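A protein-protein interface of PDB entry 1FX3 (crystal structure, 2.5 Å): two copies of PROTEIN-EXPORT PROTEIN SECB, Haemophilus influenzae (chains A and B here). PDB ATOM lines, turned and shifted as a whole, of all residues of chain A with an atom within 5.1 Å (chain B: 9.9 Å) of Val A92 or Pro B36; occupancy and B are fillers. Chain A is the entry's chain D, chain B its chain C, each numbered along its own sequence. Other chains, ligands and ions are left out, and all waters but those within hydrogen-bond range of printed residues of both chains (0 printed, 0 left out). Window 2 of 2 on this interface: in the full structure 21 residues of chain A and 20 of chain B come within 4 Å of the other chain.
Of the 16 printed residues of chain A, 5 touch a printed residue of chain B.
Printed residues of chain A that touch a printed residue of chain B: Arg A22, Tyr A24, Lys A26, Glu A64 and Val A92.
Hydrophobic or aromatic side chains of chain B within 4 Å of the printed part of chain A: Ala B32, Leu B35, Pro B36 and Phe B39.
Along chain B the printed residues that touch a printed residue of chain A span positions 32 to 131.
Among the printed residues, 11 pairs touch across the chains.
Among the printed residues, no Asp or Glu carboxylate lies within 4 Å of a Lys or Arg side-chain nitrogen of the other chain.
No position is printed for both chains.
Among the printed residues, pairs that only touch across the chains: Arg A22 with Phe B39, Tyr A24 with Leu B35, Tyr A24 with Pro B36, Tyr A24 with Phe B39, Tyr A24 with Thr B131, Glu A64 with Leu B35, Glu A64 with Pro B36 and Val A92 with Pro B36.
The backbone carbonyl oxygen (O) of Lys A26 sits at hydrogen-bond distance from the backbone NH (N) of Ala B32, at 3.0 Å.
The backbone carbonyl oxygen (O) of Leu B35 is in hydrogen-bond range of the side-chain amino group (NZ) of Lys A26 (3.1 Å).
The side-chain hydroxyl of Thr B131 lies within hydrogen-bond range of the guanidinium group of Arg A22, at 2.9 Å.
Of chain A, only Tyr A24, Glu A64 and Val A92 come within 4 Å of Pro B36.
No residue of chain B comes within 4 Å of Gly A91.
Phe A93 touches none of the printed residues of chain B.
Of the printed residues of chain A, Ala B32 touches Lys A26.
Of the printed residues of chain A, Leu B35 touches Tyr A24, Lys A26 and Glu A64.
Printed residues of chain A within 4 Å of Thr B131: Arg A22 (2.9 Å) and Tyr A24 (3.9 Å).
Printed residues of chain A within 4 Å of Phe B39: Arg A22 and Tyr A24.
Val B81 touches none of the printed residues of chain A.
Leu B75 touches none of the printed residues of chain A.
The nearest residue of chain A that does not touch Pro B36 is Val A58 (4.3 Å).
The backbone carbonyl oxygen (O) of Val A92 lies within hydrogen-bond range of the backbone NH (N) of Gln A21 (2.9 Å).
The backbone NH (N) of Val A92 is in hydrogen-bond range of the backbone carbonyl oxygen (O) of Arg A22 (2.9 Å).
The side-chain hydroxyl (OH) of Tyr A24 sits at hydrogen-bond distance from the side-chain carboxylate (OE2) of Glu A64, 2.7 Å away.
The backbone carbonyl oxygen (O) of Tyr A24 sits at hydrogen-bond distance from the backbone NH (N) of Ala A90 (2.9 Å).
The side-chain carboxylate (OE2) of Glu A64 lies within salt-bridge range of the side-chain amino group (NZ) of Lys A26.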
ATOM      1  N   GLN A  19      -6.463  -7.296  22.148  1.00  0.00           N
ATOM      2  CA  GLN A  19      -7.733  -7.902  22.551  1.00  0.00           C
ATOM      3  C   GLN A  19      -8.795  -7.815  21.445  1.00  0.00           C
ATOM      4  O   GLN A  19      -8.855  -6.833  20.693  1.00  0.00           O
ATOM      5  CB  GLN A  19      -8.250  -7.252  23.838  1.00  0.00           C
ATOM      6  N   ILE A  20      -9.615  -8.861  21.354  1.00  0.00           N
ATOM      7  CA  ILE A  20     -10.688  -8.960  20.362  1.00  0.00           C
ATOM      8  C   ILE A  20     -11.909  -8.154  20.787  1.00  0.00           C
ATOM      9  O   ILE A  20     -12.491  -8.433  21.831  1.00  0.00           O
ATOM     10  CB  ILE A  20     -11.156 -10.412  20.197  1.00  0.00           C
ATOM     11  CG1 ILE A  20      -9.968 -11.310  19.875  1.00  0.00           C
ATOM     12  CG2 ILE A  20     -12.190 -10.501  19.090  1.00  0.00           C
ATOM     13  CD1 ILE A  20     -10.331 -12.779  19.779  1.00  0.00           C
ATOM     14  N   GLN A  21     -12.314  -7.186  19.967  1.00  0.00           N
ATOM     15  CA  GLN A  21     -13.472  -6.334  20.271  1.00  0.00           C
ATOM     16  C   GLN A  21     -14.781  -6.835  19.648  1.00  0.00           C
ATOM     17  O   GLN A  21     -15.837  -6.800  20.294  1.00  0.00           O
ATOM     18  CB  GLN A  21     -13.199  -4.892  19.812  1.00  0.00           C
ATOM     19  N   ARG A  22     -14.720  -7.287  18.394  1.00  0.00           N
ATOM     20  CA  ARG A  22     -15.914  -7.787  17.716  1.00  0.00           C
ATOM     21  C   ARG A  22     -15.537  -8.782  16.634  1.00  0.00           C
ATOM     22  O   ARG A  22     -14.594  -8.553  15.881  1.00  0.00           O
ATOM     23  CB  ARG A  22     -16.724  -6.626  17.091  1.00  0.00           C
ATOM     24  CG  ARG A  22     -18.142  -7.030  16.628  1.00  0.00           C
ATOM     25  CD  ARG A  22     -18.930  -5.941  15.809  1.00  0.00           C
ATOM     26  NE  ARG A  22     -19.492  -4.899  16.654  1.00  0.00           N
ATOM     27  CZ  ARG A  22     -20.782  -4.647  16.818  1.00  0.00           C
ATOM     28  NH1 ARG A  22     -21.712  -5.348  16.185  1.00  0.00           N
ATOM     29  NH2 ARG A  22     -21.139  -3.693  17.663  1.00  0.00           N
ATOM     30  N   TYR A  24     -17.097 -10.913  13.375  1.00  0.00           N
ATOM     31  CA  TYR A  24     -18.241 -10.900  12.467  1.00  0.00           C
ATOM     32  C   TYR A  24     -17.915 -11.201  11.011  1.00  0.00           C
ATOM     33  O   TYR A  24     -16.791 -11.056  10.546  1.00  0.00           O
ATOM     34  CB  TYR A  24     -18.893  -9.531  12.527  1.00  0.00           C
ATOM     35  CG  TYR A  24     -17.927  -8.442  12.150  1.00  0.00           C
ATOM     36  CD1 TYR A  24     -17.712  -8.096  10.820  1.00  0.00           C
ATOM     37  CD2 TYR A  24     -17.162  -7.798  13.132  1.00  0.00           C
ATOM     38  CE1 TYR A  24     -16.754  -7.138  10.466  1.00  0.00           C
ATOM     39  CE2 TYR A  24     -16.206  -6.843  12.790  1.00  0.00           C
ATOM     40  CZ  TYR A  24     -16.003  -6.522  11.457  1.00  0.00           C
ATOM     41  OH  TYR A  24     -15.021  -5.614  11.138  1.00  0.00           O
ATOM     42  N   LYS A  26     -18.116 -10.481   6.971  1.00  0.00           N
ATOM     43  CA  LYS A  26     -18.296  -9.371   6.024  1.00  0.00           C
ATOM     44  C   LYS A  26     -18.972  -9.888   4.761  1.00  0.00           C
ATOM     45  O   LYS A  26     -19.649  -9.141   4.063  1.00  0.00           O
ATOM     46  CB  LYS A  26     -16.962  -8.745   5.603  1.00  0.00           C
ATOM     47  CG  LYS A  26     -16.191  -8.040   6.705  1.00  0.00           C
ATOM     48  CD  LYS A  26     -14.757  -7.720   6.275  1.00  0.00           C
ATOM     49  CE  LYS A  26     -14.660  -6.456   5.426  1.00  0.00           C
ATOM     50  NZ  LYS A  26     -15.016  -5.245   6.208  1.00  0.00           N
ATOM     51  N   VAL A  58      -8.793   0.806  11.402  1.00  0.00           N
ATOM     52  CA  VAL A  58     -10.085   1.448  11.363  1.00  0.00           C
ATOM     53  C   VAL A  58     -10.265   2.404  12.517  1.00  0.00           C
ATOM     54  O   VAL A  58     -11.341   2.969  12.702  1.00  0.00           O
ATOM     55  CB  VAL A  58     -11.206   0.387  11.342  1.00  0.00           C
ATOM     56  CG1 VAL A  58     -11.122  -0.378  10.051  1.00  0.00           C
ATOM     57  CG2 VAL A  58     -11.060  -0.592  12.521  1.00  0.00           C
ATOM     58  N   LEU A  62      -6.931   0.269  16.323  1.00  0.00           N
ATOM     59  CA  LEU A  62      -8.008  -0.627  15.963  1.00  0.00           C
ATOM     60  C   LEU A  62      -7.771  -1.124  14.565  1.00  0.00           C
ATOM     61  O   LEU A  62      -7.715  -0.338  13.614  1.00  0.00           O
ATOM     62  CB  LEU A  62      -9.358   0.088  16.048  1.00  0.00           C
ATOM     63  CG  LEU A  62      -9.844   0.399  17.468  1.00  0.00           C
ATOM     64  CD1 LEU A  62     -11.195   1.085  17.392  1.00  0.00           C
ATOM     65  CD2 LEU A  62      -9.930  -0.892  18.291  1.00  0.00           C
ATOM     66  N   TYR A  63      -7.623  -2.438  14.450  1.00  0.00           N
ATOM     67  CA  TYR A  63      -7.381  -3.057  13.161  1.00  0.00           C
ATOM     68  C   TYR A  63      -8.433  -4.094  12.810  1.00  0.00           C
ATOM     69  O   TYR A  63      -8.878  -4.843  13.675  1.00  0.00           O
ATOM     70  CB  TYR A  63      -6.002  -3.711  13.168  1.00  0.00           C
ATOM     71  CG  TYR A  63      -4.906  -2.757  13.576  1.00  0.00           C
ATOM     72  CD1 TYR A  63      -4.584  -2.572  14.918  1.00  0.00           C
ATOM     73  CD2 TYR A  63      -4.239  -1.985  12.619  1.00  0.00           C
ATOM     74  CE1 TYR A  63      -3.630  -1.639  15.303  1.00  0.00           C
ATOM     75  CE2 TYR A  63      -3.286  -1.049  12.991  1.00  0.00           C
ATOM     76  CZ  TYR A  63      -2.986  -0.879  14.334  1.00  0.00           C
ATOM     77  OH  TYR A  63      -2.053   0.059  14.711  1.00  0.00           O
ATOM     78  N   GLU A  64      -8.855  -4.122  11.546  1.00  0.00           N
ATOM     79  CA  GLU A  64      -9.822  -5.126  11.118  1.00  0.00           C
ATOM     80  C   GLU A  64      -9.090  -6.239  10.389  1.00  0.00           C
ATOM     81  O   GLU A  64      -8.657  -6.059   9.251  1.00  0.00           O
ATOM     82  CB  GLU A  64     -10.874  -4.564  10.167  1.00  0.00           C
ATOM     83  CG  GLU A  64     -11.806  -5.667   9.609  1.00  0.00           C
ATOM     84  CD  GLU A  64     -12.750  -5.170   8.522  1.00  0.00           C
ATOM     85  OE1 GLU A  64     -12.261  -4.652   7.497  1.00  0.00           O
ATOM     86  OE2 GLU A  64     -13.984  -5.300   8.687  1.00  0.00           O
ATOM     87  N   VAL A  65      -8.944  -7.384  11.045  1.00  0.00           N
ATOM     88  CA  VAL A  65      -8.287  -8.512  10.412  1.00  0.00           C
ATOM     89  C   VAL A  65      -9.335  -9.349   9.702  1.00  0.00           C
ATOM     90  O   VAL A  65     -10.306  -9.832  10.310  1.00  0.00           O
ATOM     91  CB  VAL A  65      -7.566  -9.397  11.416  1.00  0.00           C
ATOM     92  CG1 VAL A  65      -6.706 -10.381  10.670  1.00  0.00           C
ATOM     93  CG2 VAL A  65      -6.733  -8.558  12.338  1.00  0.00           C
ATOM     94  N   ALA A  90     -14.138 -12.028   9.862  1.00  0.00           N
ATOM     95  CA  ALA A  90     -13.260 -10.955  10.315  1.00  0.00           C
ATOM     96  C   ALA A  90     -13.399 -10.582  11.761  1.00  0.00           C
ATOM     97  O   ALA A  90     -14.293 -11.039  12.480  1.00  0.00           O
ATOM     98  CB  ALA A  90     -13.472  -9.703   9.466  1.00  0.00           C
ATOM     99  N   GLY A  91     -12.499  -9.710  12.178  1.00  0.00           N
ATOM    100  CA  GLY A  91     -12.537  -9.247  13.541  1.00  0.00           C
ATOM    101  C   GLY A  91     -11.870  -7.901  13.674  1.00  0.00           C
ATOM    102  O   GLY A  91     -11.007  -7.538  12.872  1.00  0.00           O
ATOM    103  N   VAL A  92     -12.297  -7.156  14.690  1.00  0.00           N
ATOM    104  CA  VAL A  92     -11.728  -5.858  15.009  1.00  0.00           C
ATOM    105  C   VAL A  92     -10.906  -6.074  16.276  1.00  0.00           C
ATOM    106  O   VAL A  92     -11.438  -6.481  17.307  1.00  0.00           O
ATOM    107  CB  VAL A  92     -12.826  -4.834  15.266  1.00  0.00           C
ATOM    108  CG1 VAL A  92     -12.298  -3.717  16.164  1.00  0.00           C
ATOM    109  CG2 VAL A  92     -13.320  -4.283  13.929  1.00  0.00           C
ATOM    110  N   PHE A  93      -9.603  -5.830  16.191  1.00  0.00           N
ATOM    111  CA  PHE A  93      -8.719  -6.029  17.339  1.00  0.00           C
ATOM    112  C   PHE A  93      -8.023  -4.748  17.789  1.00  0.00           C
ATOM    113  O   PHE A  93      -7.627  -3.910  16.966  1.00  0.00           O
ATOM    114  CB  PHE A  93      -7.634  -7.060  17.013  1.00  0.00           C
ATOM    115  CG  PHE A  93      -8.156  -8.376  16.509  1.00  0.00           C
ATOM    116  CD1 PHE A  93      -8.603  -8.509  15.206  1.00  0.00           C
ATOM    117  CD2 PHE A  93      -8.150  -9.495  17.328  1.00  0.00           C
ATOM    118  CE1 PHE A  93      -9.030  -9.736  14.724  1.00  0.00           C
ATOM    119  CE2 PHE A  93      -8.577 -10.728  16.853  1.00  0.00           C
ATOM    120  CZ  PHE A  93      -9.018 -10.846  15.545  1.00  0.00           C
ATOM    121  N   THR A  94      -7.886  -4.593  19.102  1.00  0.00           N
ATOM    122  CA  THR A  94      -7.178  -3.436  19.630  1.00  0.00           C
ATOM    123  C   THR A  94      -5.747  -3.953  19.712  1.00  0.00           C
ATOM    124  O   THR A  94      -5.485  -4.972  20.357  1.00  0.00           O
ATOM    125  CB  THR A  94      -7.679  -3.025  21.034  1.00  0.00           C
ATOM    126  OG1 THR A  94      -9.110  -2.923  21.037  1.00  0.00           O
ATOM    127  CG2 THR A  94      -7.124  -1.665  21.396  1.00  0.00           C
ATOM    128  N   ALA B  32     -22.287  -7.816   3.898  1.00  0.00           N
ATOM    129  CA  ALA B  32     -22.339  -6.697   4.850  1.00  0.00           C
ATOM    130  C   ALA B  32     -21.159  -5.794   4.497  1.00  0.00           C
ATOM    131  O   ALA B  32     -20.108  -5.819   5.138  1.00  0.00           O
ATOM    132  CB  ALA B  32     -22.207  -7.205   6.277  1.00  0.00           C
ATOM    133  N   PRO B  33     -21.345  -4.970   3.471  1.00  0.00           N
ATOM    134  CA  PRO B  33     -20.459  -3.993   2.842  1.00  0.00           C
ATOM    135  C   PRO B  33     -19.902  -2.789   3.584  1.00  0.00           C
ATOM    136  O   PRO B  33     -18.911  -2.214   3.147  1.00  0.00           O
ATOM    137  CB  PRO B  33     -21.272  -3.558   1.631  1.00  0.00           C
ATOM    138  CG  PRO B  33     -22.643  -3.566   2.169  1.00  0.00           C
ATOM    139  CD  PRO B  33     -22.681  -4.902   2.854  1.00  0.00           C
ATOM    140  N   ASN B  34     -20.515  -2.380   4.682  1.00  0.00           N
ATOM    141  CA  ASN B  34     -20.022  -1.193   5.373  1.00  0.00           C
ATOM    142  C   ASN B  34     -19.547  -1.466   6.783  1.00  0.00           C
ATOM    143  O   ASN B  34     -19.692  -0.633   7.688  1.00  0.00           O
ATOM    144  CB  ASN B  34     -21.101  -0.108   5.358  1.00  0.00           C
ATOM    145  CG  ASN B  34     -21.428   0.357   3.946  1.00  0.00           C
ATOM    146  OD1 ASN B  34     -20.566   0.889   3.253  1.00  0.00           O
ATOM    147  ND2 ASN B  34     -22.666   0.148   3.510  1.00  0.00           N
ATOM    148  N   LEU B  35     -18.965  -2.647   6.955  1.00  0.00           N
ATOM    149  CA  LEU B  35     -18.432  -3.061   8.233  1.00  0.00           C
ATOM    150  C   LEU B  35     -16.976  -2.613   8.373  1.00  0.00           C
ATOM    151  O   LEU B  35     -16.209  -2.633   7.411  1.00  0.00           O
ATOM    152  CB  LEU B  35     -18.542  -4.569   8.335  1.00  0.00           C
ATOM    153  CG  LEU B  35     -19.826  -5.059   8.989  1.00  0.00           C
ATOM    154  CD1 LEU B  35     -21.019  -4.299   8.484  1.00  0.00           C
ATOM    155  CD2 LEU B  35     -19.959  -6.532   8.725  1.00  0.00           C
ATOM    156  N   PRO B  36     -16.559  -2.232   9.585  1.00  0.00           N
ATOM    157  CA  PRO B  36     -17.288  -2.169  10.851  1.00  0.00           C
ATOM    158  C   PRO B  36     -17.859  -0.786  11.114  1.00  0.00           C
ATOM    159  O   PRO B  36     -18.407  -0.525  12.180  1.00  0.00           O
ATOM    160  CB  PRO B  36     -16.211  -2.502  11.856  1.00  0.00           C
ATOM    161  CG  PRO B  36     -15.050  -1.744  11.294  1.00  0.00           C
ATOM    162  CD  PRO B  36     -15.110  -2.099   9.823  1.00  0.00           C
ATOM    163  N   HIS B  37     -17.714   0.094  10.135  1.00  0.00           N
ATOM    164  CA  HIS B  37     -18.176   1.475  10.251  1.00  0.00           C
ATOM    165  C   HIS B  37     -19.635   1.609  10.603  1.00  0.00           C
ATOM    166  O   HIS B  37     -20.020   2.455  11.409  1.00  0.00           O
ATOM    167  CB  HIS B  37     -17.882   2.193   8.937  1.00  0.00           C
ATOM    168  CG  HIS B  37     -16.495   1.938   8.448  1.00  0.00           C
ATOM    169  ND1 HIS B  37     -15.383   2.484   9.058  1.00  0.00           N
ATOM    170  CD2 HIS B  37     -16.024   1.075   7.514  1.00  0.00           C
ATOM    171  CE1 HIS B  37     -14.291   1.964   8.526  1.00  0.00           C
ATOM    172  NE2 HIS B  37     -14.650   1.107   7.588  1.00  0.00           N
ATOM    173  N   ILE B  38     -20.442   0.757   9.995  1.00  0.00           N
ATOM    174  CA  ILE B  38     -21.873   0.785  10.187  1.00  0.00           C
ATOM    175  C   ILE B  38     -22.240   0.608  11.651  1.00  0.00           C
ATOM    176  O   ILE B  38     -23.256   1.139  12.097  1.00  0.00           O
ATOM    177  CB  ILE B  38     -22.503  -0.309   9.369  1.00  0.00           C
ATOM    178  CG1 ILE B  38     -24.005  -0.165   9.391  1.00  0.00           C
ATOM    179  CG2 ILE B  38     -22.041  -1.647   9.873  1.00  0.00           C
ATOM    180  CD1 ILE B  38     -24.512   0.587   8.208  1.00  0.00           C
ATOM    181  N   PHE B  39     -21.419  -0.135  12.399  1.00  0.00           N
ATOM    182  CA  PHE B  39     -21.672  -0.359  13.827  1.00  0.00           C
ATOM    183  C   PHE B  39     -21.607   0.952  14.613  1.00  0.00           C
ATOM    184  O   PHE B  39     -21.896   0.972  15.803  1.00  0.00           O
ATOM    185  CB  PHE B  39     -20.651  -1.325  14.442  1.00  0.00           C
ATOM    186  CG  PHE B  39     -20.568  -2.648  13.759  1.00  0.00           C
ATOM    187  CD1 PHE B  39     -19.319  -3.200  13.446  1.00  0.00           C
ATOM    188  CD2 PHE B  39     -21.714  -3.361  13.431  1.00  0.00           C
ATOM    189  CE1 PHE B  39     -19.216  -4.467  12.805  1.00  0.00           C
ATOM    190  CE2 PHE B  39     -21.627  -4.622  12.795  1.00  0.00           C
ATOM    191  CZ  PHE B  39     -20.371  -5.175  12.481  1.00  0.00           C
ATOM    192  N   GLN B  40     -21.199   2.038  13.967  1.00  0.00           N
ATOM    193  CA  GLN B  40     -21.139   3.336  14.646  1.00  0.00           C
ATOM    194  C   GLN B  40     -22.417   4.128  14.395  1.00  0.00           C
ATOM    195  O   GLN B  40     -22.587   5.195  14.971  1.00  0.00           O
ATOM    196  CB  GLN B  40     -19.947   4.167  14.170  1.00  0.00           C
ATOM    197  CG  GLN B  40     -18.717   4.152  15.061  1.00  0.00           C
ATOM    198  CD  GLN B  40     -17.770   5.305  14.736  1.00  0.00           C
ATOM    199  OE1 GLN B  40     -18.195   6.458  14.576  1.00  0.00           O
ATOM    200  NE2 GLN B  40     -16.488   5.000  14.640  1.00  0.00           N
ATOM    201  N   GLN B  41     -23.297   3.608  13.529  1.00  0.00           N
ATOM    202  CA  GLN B  41     -24.566   4.261  13.211  1.00  0.00           C
ATOM    203  C   GLN B  41     -25.668   3.773  14.122  1.00  0.00           C
ATOM    204  O   GLN B  41     -25.585   2.686  14.665  1.00  0.00           O
ATOM    205  CB  GLN B  41     -24.968   4.001  11.757  1.00  0.00           C
ATOM    206  CG  GLN B  41     -23.932   4.553  10.786  1.00  0.00           C
ATOM    207  CD  GLN B  41     -24.180   4.214   9.315  1.00  0.00           C
ATOM    208  OE1 GLN B  41     -23.255   4.168   8.526  1.00  0.00           O
ATOM    209  NE2 GLN B  41     -25.417   4.020   8.947  1.00  0.00           N
ATOM    210  N   LEU B  75     -29.838   1.619   6.835  1.00  0.00           N
ATOM    211  CA  LEU B  75     -30.057   2.417   8.044  1.00  0.00           C
ATOM    212  C   LEU B  75     -30.496   3.808   7.586  1.00  0.00           C
ATOM    213  O   LEU B  75     -29.867   4.419   6.716  1.00  0.00           O
ATOM    214  CB  LEU B  75     -28.779   2.469   8.889  1.00  0.00           C
ATOM    215  CG  LEU B  75     -28.371   1.060   9.357  1.00  0.00           C
ATOM    216  CD1 LEU B  75     -27.150   1.137  10.252  1.00  0.00           C
ATOM    217  CD2 LEU B  75     -29.516   0.402  10.109  1.00  0.00           C
ATOM    218  N   ASP B  80     -26.939   3.963   4.135  1.00  0.00           N
ATOM    219  CA  ASP B  80     -26.031   2.819   3.948  1.00  0.00           C
ATOM    220  C   ASP B  80     -26.660   1.448   4.110  1.00  0.00           C
ATOM    221  O   ASP B  80     -27.607   1.258   4.891  1.00  0.00           O
ATOM    222  CB  ASP B  80     -24.864   2.883   4.927  1.00  0.00           C
ATOM    223  CG  ASP B  80     -23.917   4.005   4.625  1.00  0.00           C
ATOM    224  OD1 ASP B  80     -23.902   4.477   3.462  1.00  0.00           O
ATOM    225  OD2 ASP B  80     -23.176   4.396   5.553  1.00  0.00           O
ATOM    226  N   VAL B  81     -26.097   0.485   3.395  1.00  0.00           N
ATOM    227  CA  VAL B  81     -26.576  -0.894   3.454  1.00  0.00           C
ATOM    228  C   VAL B  81     -25.999  -1.660   4.652  1.00  0.00           C
ATOM    229  O   VAL B  81     -24.794  -1.793   4.790  1.00  0.00           O
ATOM    230  CB  VAL B  81     -26.186  -1.656   2.176  1.00  0.00           C
ATOM    231  CG1 VAL B  81     -26.435  -3.154   2.358  1.00  0.00           C
ATOM    232  CG2 VAL B  81     -26.990  -1.140   1.009  1.00  0.00           C
ATOM    233  N   ALA B  82     -26.848  -2.165   5.530  1.00  0.00           N
ATOM    234  CA  ALA B  82     -26.336  -2.913   6.658  1.00  0.00           C
ATOM    235  C   ALA B  82     -26.006  -4.353   6.200  1.00  0.00           C
ATOM    236  O   ALA B  82     -24.945  -4.904   6.508  1.00  0.00           O
ATOM    237  CB  ALA B  82     -27.365  -2.923   7.792  1.00  0.00           C
ATOM    238  N   GLY B 130     -23.281 -11.390  11.398  1.00  0.00           N
ATOM    239  CA  GLY B 130     -22.840 -10.052  11.059  1.00  0.00           C
ATOM    240  C   GLY B 130     -22.990  -9.190  12.313  1.00  0.00           C
ATOM    241  O   GLY B 130     -22.684  -8.006  12.298  1.00  0.00           O
ATOM    242  N   THR B 131     -23.471  -9.807  13.393  1.00  0.00           N
ATOM    243  CA  THR B 131     -23.677  -9.154  14.684  1.00  0.00           C
ATOM    244  C   THR B 131     -24.667  -8.001  14.588  1.00  0.00           C
ATOM    245  O   THR B 131     -24.461  -6.953  15.186  1.00  0.00           O
ATOM    246  CB  THR B 131     -22.336  -8.615  15.310  1.00  0.00           C
ATOM    247  OG1 THR B 131     -21.754  -7.631  14.441  1.00  0.00           O
ATOM    248  CG2 THR B 131     -21.330  -9.748  15.522  1.00  0.00           C
ATOM    249  N   PHE B 132     -25.728  -8.181  13.809  1.00  0.00           N
ATOM    250  CA  PHE B 132     -26.741  -7.156  13.711  1.00  0.00           C
ATOM    251  C   PHE B 132     -27.927  -7.638  14.523  1.00  0.00           C
ATOM    252  O   PHE B 132     -28.053  -8.810  14.813  1.00  0.00           O
ATOM    253  CB  PHE B 132     -27.207  -6.965  12.274  1.00  0.00           C
ATOM    254  CG  PHE B 132     -26.135  -6.555  11.325  1.00  0.00           C
ATOM    255  CD1 PHE B 132     -25.647  -7.447  10.382  1.00  0.00           C
ATOM    256  CD2 PHE B 132     -25.643  -5.262  11.333  1.00  0.00           C
ATOM    257  CE1 PHE B 132     -24.690  -7.048   9.457  1.00  0.00           C
ATOM    258  CE2 PHE B 132     -24.684  -4.856  10.415  1.00  0.00           C
ATOM    259  CZ  PHE B 132     -24.209  -5.746   9.475  1.00  0.00           C
